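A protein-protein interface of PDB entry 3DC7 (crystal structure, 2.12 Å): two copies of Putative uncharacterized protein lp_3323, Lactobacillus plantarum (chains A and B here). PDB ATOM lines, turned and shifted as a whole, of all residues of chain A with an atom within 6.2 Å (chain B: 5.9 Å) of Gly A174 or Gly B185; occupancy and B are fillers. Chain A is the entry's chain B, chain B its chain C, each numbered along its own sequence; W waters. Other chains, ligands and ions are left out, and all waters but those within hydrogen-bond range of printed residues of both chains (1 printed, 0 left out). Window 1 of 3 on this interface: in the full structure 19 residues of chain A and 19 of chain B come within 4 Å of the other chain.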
ATOM      1  N   GLN A 124       0.262  -9.895  18.557  1.00  0.00           N
ATOM      2  CA  GLN A 124      -1.132  -9.982  18.129  1.00  0.00           C
ATOM      3  C   GLN A 124      -1.256 -10.618  16.736  1.00  0.00           C
ATOM      4  O   GLN A 124      -2.230 -11.312  16.453  1.00  0.00           O
ATOM      5  CB  GLN A 124      -1.829  -8.618  18.201  1.00  0.00           C
ATOM      6  CG  GLN A 124      -1.961  -8.023  19.628  1.00  0.00           C
ATOM      7  CD  GLN A 124      -3.072  -8.658  20.457  1.00  0.00           C
ATOM      8  OE1 GLN A 124      -3.963  -7.964  20.965  1.00  0.00           O
ATOM      9  NE2 GLN A 124      -3.038  -9.965  20.590  1.00  0.00           N
ATOM     10  N   PRO A 128      -3.018 -14.602  17.681  1.00  0.00           N
ATOM     11  CA  PRO A 128      -4.209 -13.764  17.690  1.00  0.00           C
ATOM     12  C   PRO A 128      -5.292 -14.197  18.669  1.00  0.00           C
ATOM     13  O   PRO A 128      -6.042 -13.349  19.141  1.00  0.00           O
ATOM     14  CB  PRO A 128      -4.722 -13.858  16.246  1.00  0.00           C
ATOM     15  CG  PRO A 128      -4.157 -15.129  15.724  1.00  0.00           C
ATOM     16  CD  PRO A 128      -2.827 -15.267  16.374  1.00  0.00           C
ATOM     17  N   VAL A 130      -4.773 -15.912  21.564  1.00  0.00           N
ATOM     18  CA  VAL A 130      -4.172 -16.252  22.835  1.00  0.00           C
ATOM     19  C   VAL A 130      -4.314 -15.110  23.844  1.00  0.00           C
ATOM     20  O   VAL A 130      -3.961 -13.972  23.526  1.00  0.00           O
ATOM     21  CB  VAL A 130      -2.672 -16.639  22.650  1.00  0.00           C
ATOM     22  CG1 VAL A 130      -2.021 -16.931  23.999  1.00  0.00           C
ATOM     23  CG2 VAL A 130      -2.535 -17.855  21.714  1.00  0.00           C
ATOM     24  N   LYS A 132      -3.262 -12.636  26.724  1.00  0.00           N
ATOM     25  CA  LYS A 132      -1.943 -12.106  27.002  1.00  0.00           C
ATOM     26  C   LYS A 132      -2.039 -10.825  27.799  1.00  0.00           C
ATOM     27  O   LYS A 132      -3.060 -10.148  27.783  1.00  0.00           O
ATOM     28  CB  LYS A 132      -1.100 -11.927  25.711  1.00  0.00           C
ATOM     29  CG  LYS A 132      -1.752 -11.175  24.577  1.00  0.00           C
ATOM     30  CD  LYS A 132      -0.853 -11.143  23.324  1.00  0.00           C
ATOM     31  CE  LYS A 132      -1.150 -12.304  22.348  1.00  0.00           C
ATOM     32  NZ  LYS A 132      -2.564 -12.286  21.813  1.00  0.00           N
ATOM     33  N   MET A 169       0.617   2.127  24.983  1.00  0.00           N
ATOM     34  CA  MET A 169       0.856   1.229  23.867  1.00  0.00           C
ATOM     35  C   MET A 169       0.007  -0.025  23.970  1.00  0.00           C
ATOM     36  O   MET A 169      -0.575  -0.452  22.978  1.00  0.00           O
ATOM     37  CB  MET A 169       2.339   0.860  23.763  1.00  0.00           C
ATOM     38  CG  MET A 169       3.231   2.001  23.279  1.00  0.00           C
ATOM     39  SD  MET A 169       2.606   2.815  21.604  1.00  0.00           S
ATOM     40  CE  MET A 169       2.681   1.267  20.449  1.00  0.00           C
ATOM     41  N   THR A 170      -0.059  -0.617  25.160  1.00  0.00           N
ATOM     42  CA  THR A 170      -0.856  -1.818  25.330  1.00  0.00           C
ATOM     43  C   THR A 170      -2.283  -1.521  24.928  1.00  0.00           C
ATOM     44  O   THR A 170      -2.905  -2.326  24.254  1.00  0.00           O
ATOM     45  CB  THR A 170      -0.828  -2.389  26.771  1.00  0.00           C
ATOM     46  OG1 THR A 170      -1.178  -1.369  27.723  1.00  0.00           O
ATOM     47  CG2 THR A 170       0.522  -2.979  27.089  1.00  0.00           C
ATOM     48  N   ALA A 171      -2.775  -0.340  25.303  1.00  0.00           N
ATOM     49  CA  ALA A 171      -4.167   0.023  25.072  1.00  0.00           C
ATOM     50  C   ALA A 171      -4.521   0.004  23.593  1.00  0.00           C
ATOM     51  O   ALA A 171      -5.587  -0.494  23.217  1.00  0.00           O
ATOM     52  CB  ALA A 171      -4.496   1.379  25.693  1.00  0.00           C
ATOM     53  N   ASP A 172      -3.632   0.530  22.757  1.00  0.00           N
ATOM     54  CA  ASP A 172      -3.872   0.565  21.301  1.00  0.00           C
ATOM     55  C   ASP A 172      -4.015  -0.806  20.629  1.00  0.00           C
ATOM     56  O   ASP A 172      -4.508  -0.903  19.510  1.00  0.00           O
ATOM     57  CB  ASP A 172      -2.784   1.376  20.599  1.00  0.00           C
ATOM     58  CG  ASP A 172      -2.881   2.837  20.913  1.00  0.00           C
ATOM     59  OD1 ASP A 172      -4.024   3.364  20.987  1.00  0.00           O
ATOM     60  OD2 ASP A 172      -1.815   3.454  21.112  1.00  0.00           O
ATOM     61  N   TYR A 173      -3.579  -1.856  21.315  1.00  0.00           N
ATOM     62  CA  TYR A 173      -3.714  -3.219  20.809  1.00  0.00           C
ATOM     63  C   TYR A 173      -4.693  -4.047  21.633  1.00  0.00           C
ATOM     64  O   TYR A 173      -4.800  -5.255  21.440  1.00  0.00           O
ATOM     65  CB  TYR A 173      -2.338  -3.894  20.781  1.00  0.00           C
ATOM     66  CG  TYR A 173      -1.384  -3.237  19.811  1.00  0.00           C
ATOM     67  CD1 TYR A 173      -0.654  -2.102  20.178  1.00  0.00           C
ATOM     68  CD2 TYR A 173      -1.221  -3.738  18.519  1.00  0.00           C
ATOM     69  CE1 TYR A 173       0.205  -1.487  19.290  1.00  0.00           C
ATOM     70  CE2 TYR A 173      -0.361  -3.124  17.617  1.00  0.00           C
ATOM     71  CZ  TYR A 173       0.346  -2.004  18.013  1.00  0.00           C
ATOM     72  OH  TYR A 173       1.210  -1.407  17.133  1.00  0.00           O
ATOM     73  N   GLY A 174      -5.392  -3.403  22.564  1.00  0.00           N
ATOM     74  CA  GLY A 174      -6.341  -4.100  23.432  1.00  0.00           C
ATOM     75  C   GLY A 174      -5.740  -5.086  24.423  1.00  0.00           C
ATOM     76  O   GLY A 174      -6.448  -5.961  24.941  1.00  0.00           O
ATOM     77  N   VAL A 175      -4.447  -4.942  24.703  1.00  0.00           N
ATOM     78  CA  VAL A 175      -3.749  -5.850  25.620  1.00  0.00           C
ATOM     79  C   VAL A 175      -3.869  -5.355  27.072  1.00  0.00           C
ATOM     80  O   VAL A 175      -3.445  -4.243  27.374  1.00  0.00           O
ATOM     81  CB  VAL A 175      -2.272  -6.033  25.205  1.00  0.00           C
ATOM     82  CG1 VAL A 175      -1.493  -6.843  26.249  1.00  0.00           C
ATOM     83  CG2 VAL A 175      -2.216  -6.727  23.850  1.00  0.00           C
ATOM     84  N   PRO A 176      -4.496  -6.163  27.952  1.00  0.00           N
ATOM     85  CA  PRO A 176      -4.587  -5.800  29.367  1.00  0.00           C
ATOM     86  C   PRO A 176      -3.215  -5.507  29.976  1.00  0.00           C
ATOM     87  O   PRO A 176      -2.221  -6.157  29.630  1.00  0.00           O
ATOM     88  CB  PRO A 176      -5.197  -7.038  30.028  1.00  0.00           C
ATOM     89  CG  PRO A 176      -5.709  -7.890  28.943  1.00  0.00           C
ATOM     90  CD  PRO A 176      -5.185  -7.429  27.638  1.00  0.00           C
ATOM     91  N   LEU B 180     -13.431  -1.977  25.841  1.00  0.00           N
ATOM     92  CA  LEU B 180     -12.997  -3.062  24.960  1.00  0.00           C
ATOM     93  C   LEU B 180     -11.778  -2.599  24.165  1.00  0.00           C
ATOM     94  O   LEU B 180     -10.854  -3.375  23.905  1.00  0.00           O
ATOM     95  CB  LEU B 180     -14.120  -3.508  24.009  1.00  0.00           C
ATOM     96  CG  LEU B 180     -15.449  -3.956  24.625  1.00  0.00           C
ATOM     97  CD1 LEU B 180     -16.511  -4.214  23.533  1.00  0.00           C
ATOM     98  CD2 LEU B 180     -15.276  -5.183  25.518  1.00  0.00           C
ATOM     99  N   TYR B 181     -11.767  -1.317  23.816  1.00  0.00           N
ATOM    100  CA  TYR B 181     -10.613  -0.704  23.190  1.00  0.00           C
ATOM    101  C   TYR B 181      -9.280  -1.097  23.851  1.00  0.00           C
ATOM    102  O   TYR B 181      -8.380  -1.597  23.189  1.00  0.00           O
ATOM    103  CB  TYR B 181     -10.750   0.819  23.171  1.00  0.00           C
ATOM    104  CG  TYR B 181      -9.661   1.475  22.346  1.00  0.00           C
ATOM    105  CD1 TYR B 181      -8.430   1.779  22.913  1.00  0.00           C
ATOM    106  CD2 TYR B 181      -9.860   1.772  20.999  1.00  0.00           C
ATOM    107  CE1 TYR B 181      -7.427   2.380  22.174  1.00  0.00           C
ATOM    108  CE2 TYR B 181      -8.862   2.363  20.247  1.00  0.00           C
ATOM    109  CZ  TYR B 181      -7.645   2.666  20.839  1.00  0.00           C
ATOM    110  OH  TYR B 181      -6.626   3.249  20.109  1.00  0.00           O
ATOM    111  N   ARG B 182      -9.156  -0.863  25.150  1.00  0.00           N
ATOM    112  CA  ARG B 182      -7.907  -1.173  25.829  1.00  0.00           C
ATOM    113  C   ARG B 182      -7.833  -2.601  26.378  1.00  0.00           C
ATOM    114  O   ARG B 182      -6.741  -3.069  26.678  1.00  0.00           O
ATOM    115  CB  ARG B 182      -7.572  -0.104  26.895  1.00  0.00           C
ATOM    116  CG  ARG B 182      -8.031  -0.344  28.304  1.00  0.00           C
ATOM    117  CD  ARG B 182      -6.972  -1.060  29.161  1.00  0.00           C
ATOM    118  NE  ARG B 182      -5.715  -0.317  29.321  1.00  0.00           N
ATOM    119  CZ  ARG B 182      -4.529  -0.692  28.823  1.00  0.00           C
ATOM    120  NH1 ARG B 182      -4.408  -1.814  28.113  1.00  0.00           N
ATOM    121  NH2 ARG B 182      -3.463   0.072  29.036  1.00  0.00           N
ATOM    122  N   ASP B 183      -8.970  -3.288  26.504  1.00  0.00           N
ATOM    123  CA  ASP B 183      -9.019  -4.545  27.276  1.00  0.00           C
ATOM    124  C   ASP B 183      -9.603  -5.769  26.594  1.00  0.00           C
ATOM    125  O   ASP B 183      -9.614  -6.849  27.199  1.00  0.00           O
ATOM    126  CB  ASP B 183      -9.776  -4.341  28.600  1.00  0.00           C
ATOM    127  CG  ASP B 183      -8.886  -3.815  29.712  1.00  0.00           C
ATOM    128  OD1 ASP B 183      -7.717  -4.253  29.816  1.00  0.00           O
ATOM    129  OD2 ASP B 183      -9.354  -2.942  30.486  1.00  0.00           O
ATOM    130  N   ALA B 184     -10.101  -5.624  25.365  1.00  0.00           N
ATOM    131  CA  ALA B 184     -10.722  -6.750  24.659  1.00  0.00           C
ATOM    132  C   ALA B 184      -9.757  -7.915  24.364  1.00  0.00           C
ATOM    133  O   ALA B 184     -10.199  -9.049  24.137  1.00  0.00           O
ATOM    134  CB  ALA B 184     -11.382  -6.273  23.377  1.00  0.00           C
ATOM    135  N   GLY B 185      -8.452  -7.640  24.367  1.00  0.00           N
ATOM    136  CA  GLY B 185      -7.457  -8.659  24.041  1.00  0.00           C
ATOM    137  C   GLY B 185      -7.197  -8.687  22.538  1.00  0.00           C
ATOM    138  O   GLY B 185      -6.386  -9.468  22.047  1.00  0.00           O
ATOM    139  N   MET B 186      -7.901  -7.827  21.813  1.00  0.00           N
ATOM    140  CA  MET B 186      -7.794  -7.786  20.371  1.00  0.00           C
ATOM    141  C   MET B 186      -8.032  -6.403  19.803  1.00  0.00           C
ATOM    142  O   MET B 186      -8.591  -5.512  20.450  1.00  0.00           O
ATOM    143  CB  MET B 186      -8.771  -8.766  19.714  1.00  0.00           C
ATOM    144  CG  MET B 186     -10.195  -8.235  19.647  1.00  0.00           C
ATOM    145  SD  MET B 186     -11.480  -9.665  19.453  1.00  0.00           S
ATOM    146  CE  MET B 186     -10.612 -10.977  20.646  1.00  0.00           C
ATOM    147  N   THR B 187      -7.583  -6.270  18.563  1.00  0.00           N
ATOM    148  CA  THR B 187      -7.738  -5.083  17.771  1.00  0.00           C
ATOM    149  C   THR B 187      -8.035  -5.519  16.336  1.00  0.00           C
ATOM    150  O   THR B 187      -7.426  -6.470  15.822  1.00  0.00           O
ATOM    151  CB  THR B 187      -6.496  -4.166  17.859  1.00  0.00           C
ATOM    152  OG1 THR B 187      -6.478  -3.267  16.749  1.00  0.00           O
ATOM    153  CG2 THR B 187      -5.175  -4.955  17.872  1.00  0.00           C
ATOM    154  N   GLN B 193      -6.206 -10.878  13.641  1.00  0.00           N
ATOM    155  CA  GLN B 193      -7.366 -10.834  14.542  1.00  0.00           C
ATOM    156  C   GLN B 193      -8.667 -10.339  13.901  1.00  0.00           C
ATOM    157  O   GLN B 193      -9.756 -10.842  14.229  1.00  0.00           O
ATOM    158  CB  GLN B 193      -7.053 -10.002  15.777  1.00  0.00           C
ATOM    159  CG  GLN B 193      -5.860 -10.514  16.525  1.00  0.00           C
ATOM    160  CD  GLN B 193      -5.698  -9.846  17.862  1.00  0.00           C
ATOM    161  OE1 GLN B 193      -5.696 -10.516  18.906  1.00  0.00           O
ATOM    162  NE2 GLN B 193      -5.584  -8.515  17.853  1.00  0.00           N
ATOM    163  N   LYS B 215     -15.944 -10.528  28.166  1.00  0.00           N
ATOM    164  CA  LYS B 215     -15.375  -9.364  28.816  1.00  0.00           C
ATOM    165  C   LYS B 215     -16.410  -8.585  29.626  1.00  0.00           C
ATOM    166  O   LYS B 215     -16.124  -8.142  30.733  1.00  0.00           O
ATOM    167  CB  LYS B 215     -14.715  -8.466  27.771  1.00  0.00           C
ATOM    168  CG  LYS B 215     -13.592  -9.139  27.021  1.00  0.00           C
ATOM    169  CD  LYS B 215     -12.448  -9.531  27.959  1.00  0.00           C
ATOM    170  CE  LYS B 215     -11.573 -10.593  27.325  1.00  0.00           C
ATOM    171  NZ  LYS B 215     -10.448 -10.986  28.223  1.00  0.00           N
HETATM  172  O   HOH W   1      -4.159  -1.721  17.107  1.00  0.00           O
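The side-chain amino group (NZ) of Lys A132 lies close to the side-chain amide nitrogen (NE2) of Gln A124. The backbone carbonyl oxygen (O) of Tyr A173 sits close to the side-chain amide oxygen (OE1) of Gln A124 (2.9 Å). O of Thr A170 lies within hydrogen-bond range of N of Val A175. The side-chain amide oxygen (OE1) of Gln B193 sits close to the backbone carbonyl oxygen (O) of Gly B185, at 3.4 Å. The backbone NH (N) of Thr B187 lies close to the side-chain amide nitrogen (NE2) of Gln B193, at 3.1 Å.
No position is printed for both chains.
Hydrophobic or aromatic side chains of chain A within 4 Å of the printed part of chain B: Pro A128, Ala A171 and Pro A176. Along chain A the printed residues that touch a printed residue of chain B span positions 124 to 176.
Met A169 touches none of the printed residues of chain B. Of chain B, only Tyr B181 (3.2 Å), Arg B182 (3.2 Å), Asp B183 (3.6 Å), Ala B184 (3.7 Å), Gly B185 (2.7 Å) and Met B186 (3.9 Å) come within 4 Å of Gly A174. Of the printed residues of chain A, Arg B182 touches Thr A170, Ala A171, Gly A174 and Val A175. Of the printed residues of chain A, Asp B183 touches Gly A174 (3.6 Å) and Pro A176 (3.5 Å). Printed residues of chain A within 4 Å of Gln B193: Gln A124 (3.2 Å) and Pro A128 (2.9 Å). The nearest printed residue of chain A that does not touch Asp B183 is Val A175 (4.9 Å).
Among the printed residues, merely in contact across the chains: Gly A174 with Tyr B181 (3.2 Å), Pro A176 with Asp B183 (3.5 Å), Ala A171 with Arg B182 (3.6 Å), Gly A174 with Asp B183 (3.6 Å), Tyr A173 with Thr B187 (3.6 Å), Gly A174 with Ala B184 (3.7 Å), Tyr A173 with Met B186 (3.8 Å), Gln A124 with Met B186 (3.9 Å) and Gly A174 with Met B186 (3.9 Å).
The side-chain amide oxygen (OE1) of Gln A124 sits close to the backbone carbonyl oxygen (O) of Gly B185, at 3.1 Å. The side-chain amide oxygen of Gln B193 lies within hydrogen-bond range of the side-chain amide nitrogen of Gln A124, at 3.2 Å. The backbone carbonyl oxygen (O) of Pro A128 lies close to the side-chain amide oxygen (OE1) of Gln B193, 2.9 Å away. The guanidinium group (NH2) of Arg B182 sits at hydrogen-bond distance from the side-chain hydroxyl (OG1) of Thr A170 (3.0 Å). The side-chain hydroxyl (OH) of Tyr B181 is in hydrogen-bond range of the side-chain carboxylate (OD1) of Asp A172 (2.7 Å). The backbone carbonyl oxygen of Gly A174 lies within hydrogen-bond range of the backbone NH of Gly B185, at 2.7 Å. The backbone carbonyl oxygen (O) of Val A175 is in hydrogen-bond range of the guanidinium group (NH1) of Arg B182 (2.7 Å). The backbone carbonyl oxygen of Ala A171 lies close to the backbone carbonyl oxygen of Tyr B181 (3.0 Å). The backbone carbonyl oxygen (O) of Arg B182 lies close to the backbone carbonyl oxygen (O) of Gly A174, 3.4 Å away.
Water W1 bridges the backbone carbonyl oxygen of Asp A172 (2.6 Å) and the side-chain hydroxyl of Thr B187 (2.8 Å).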
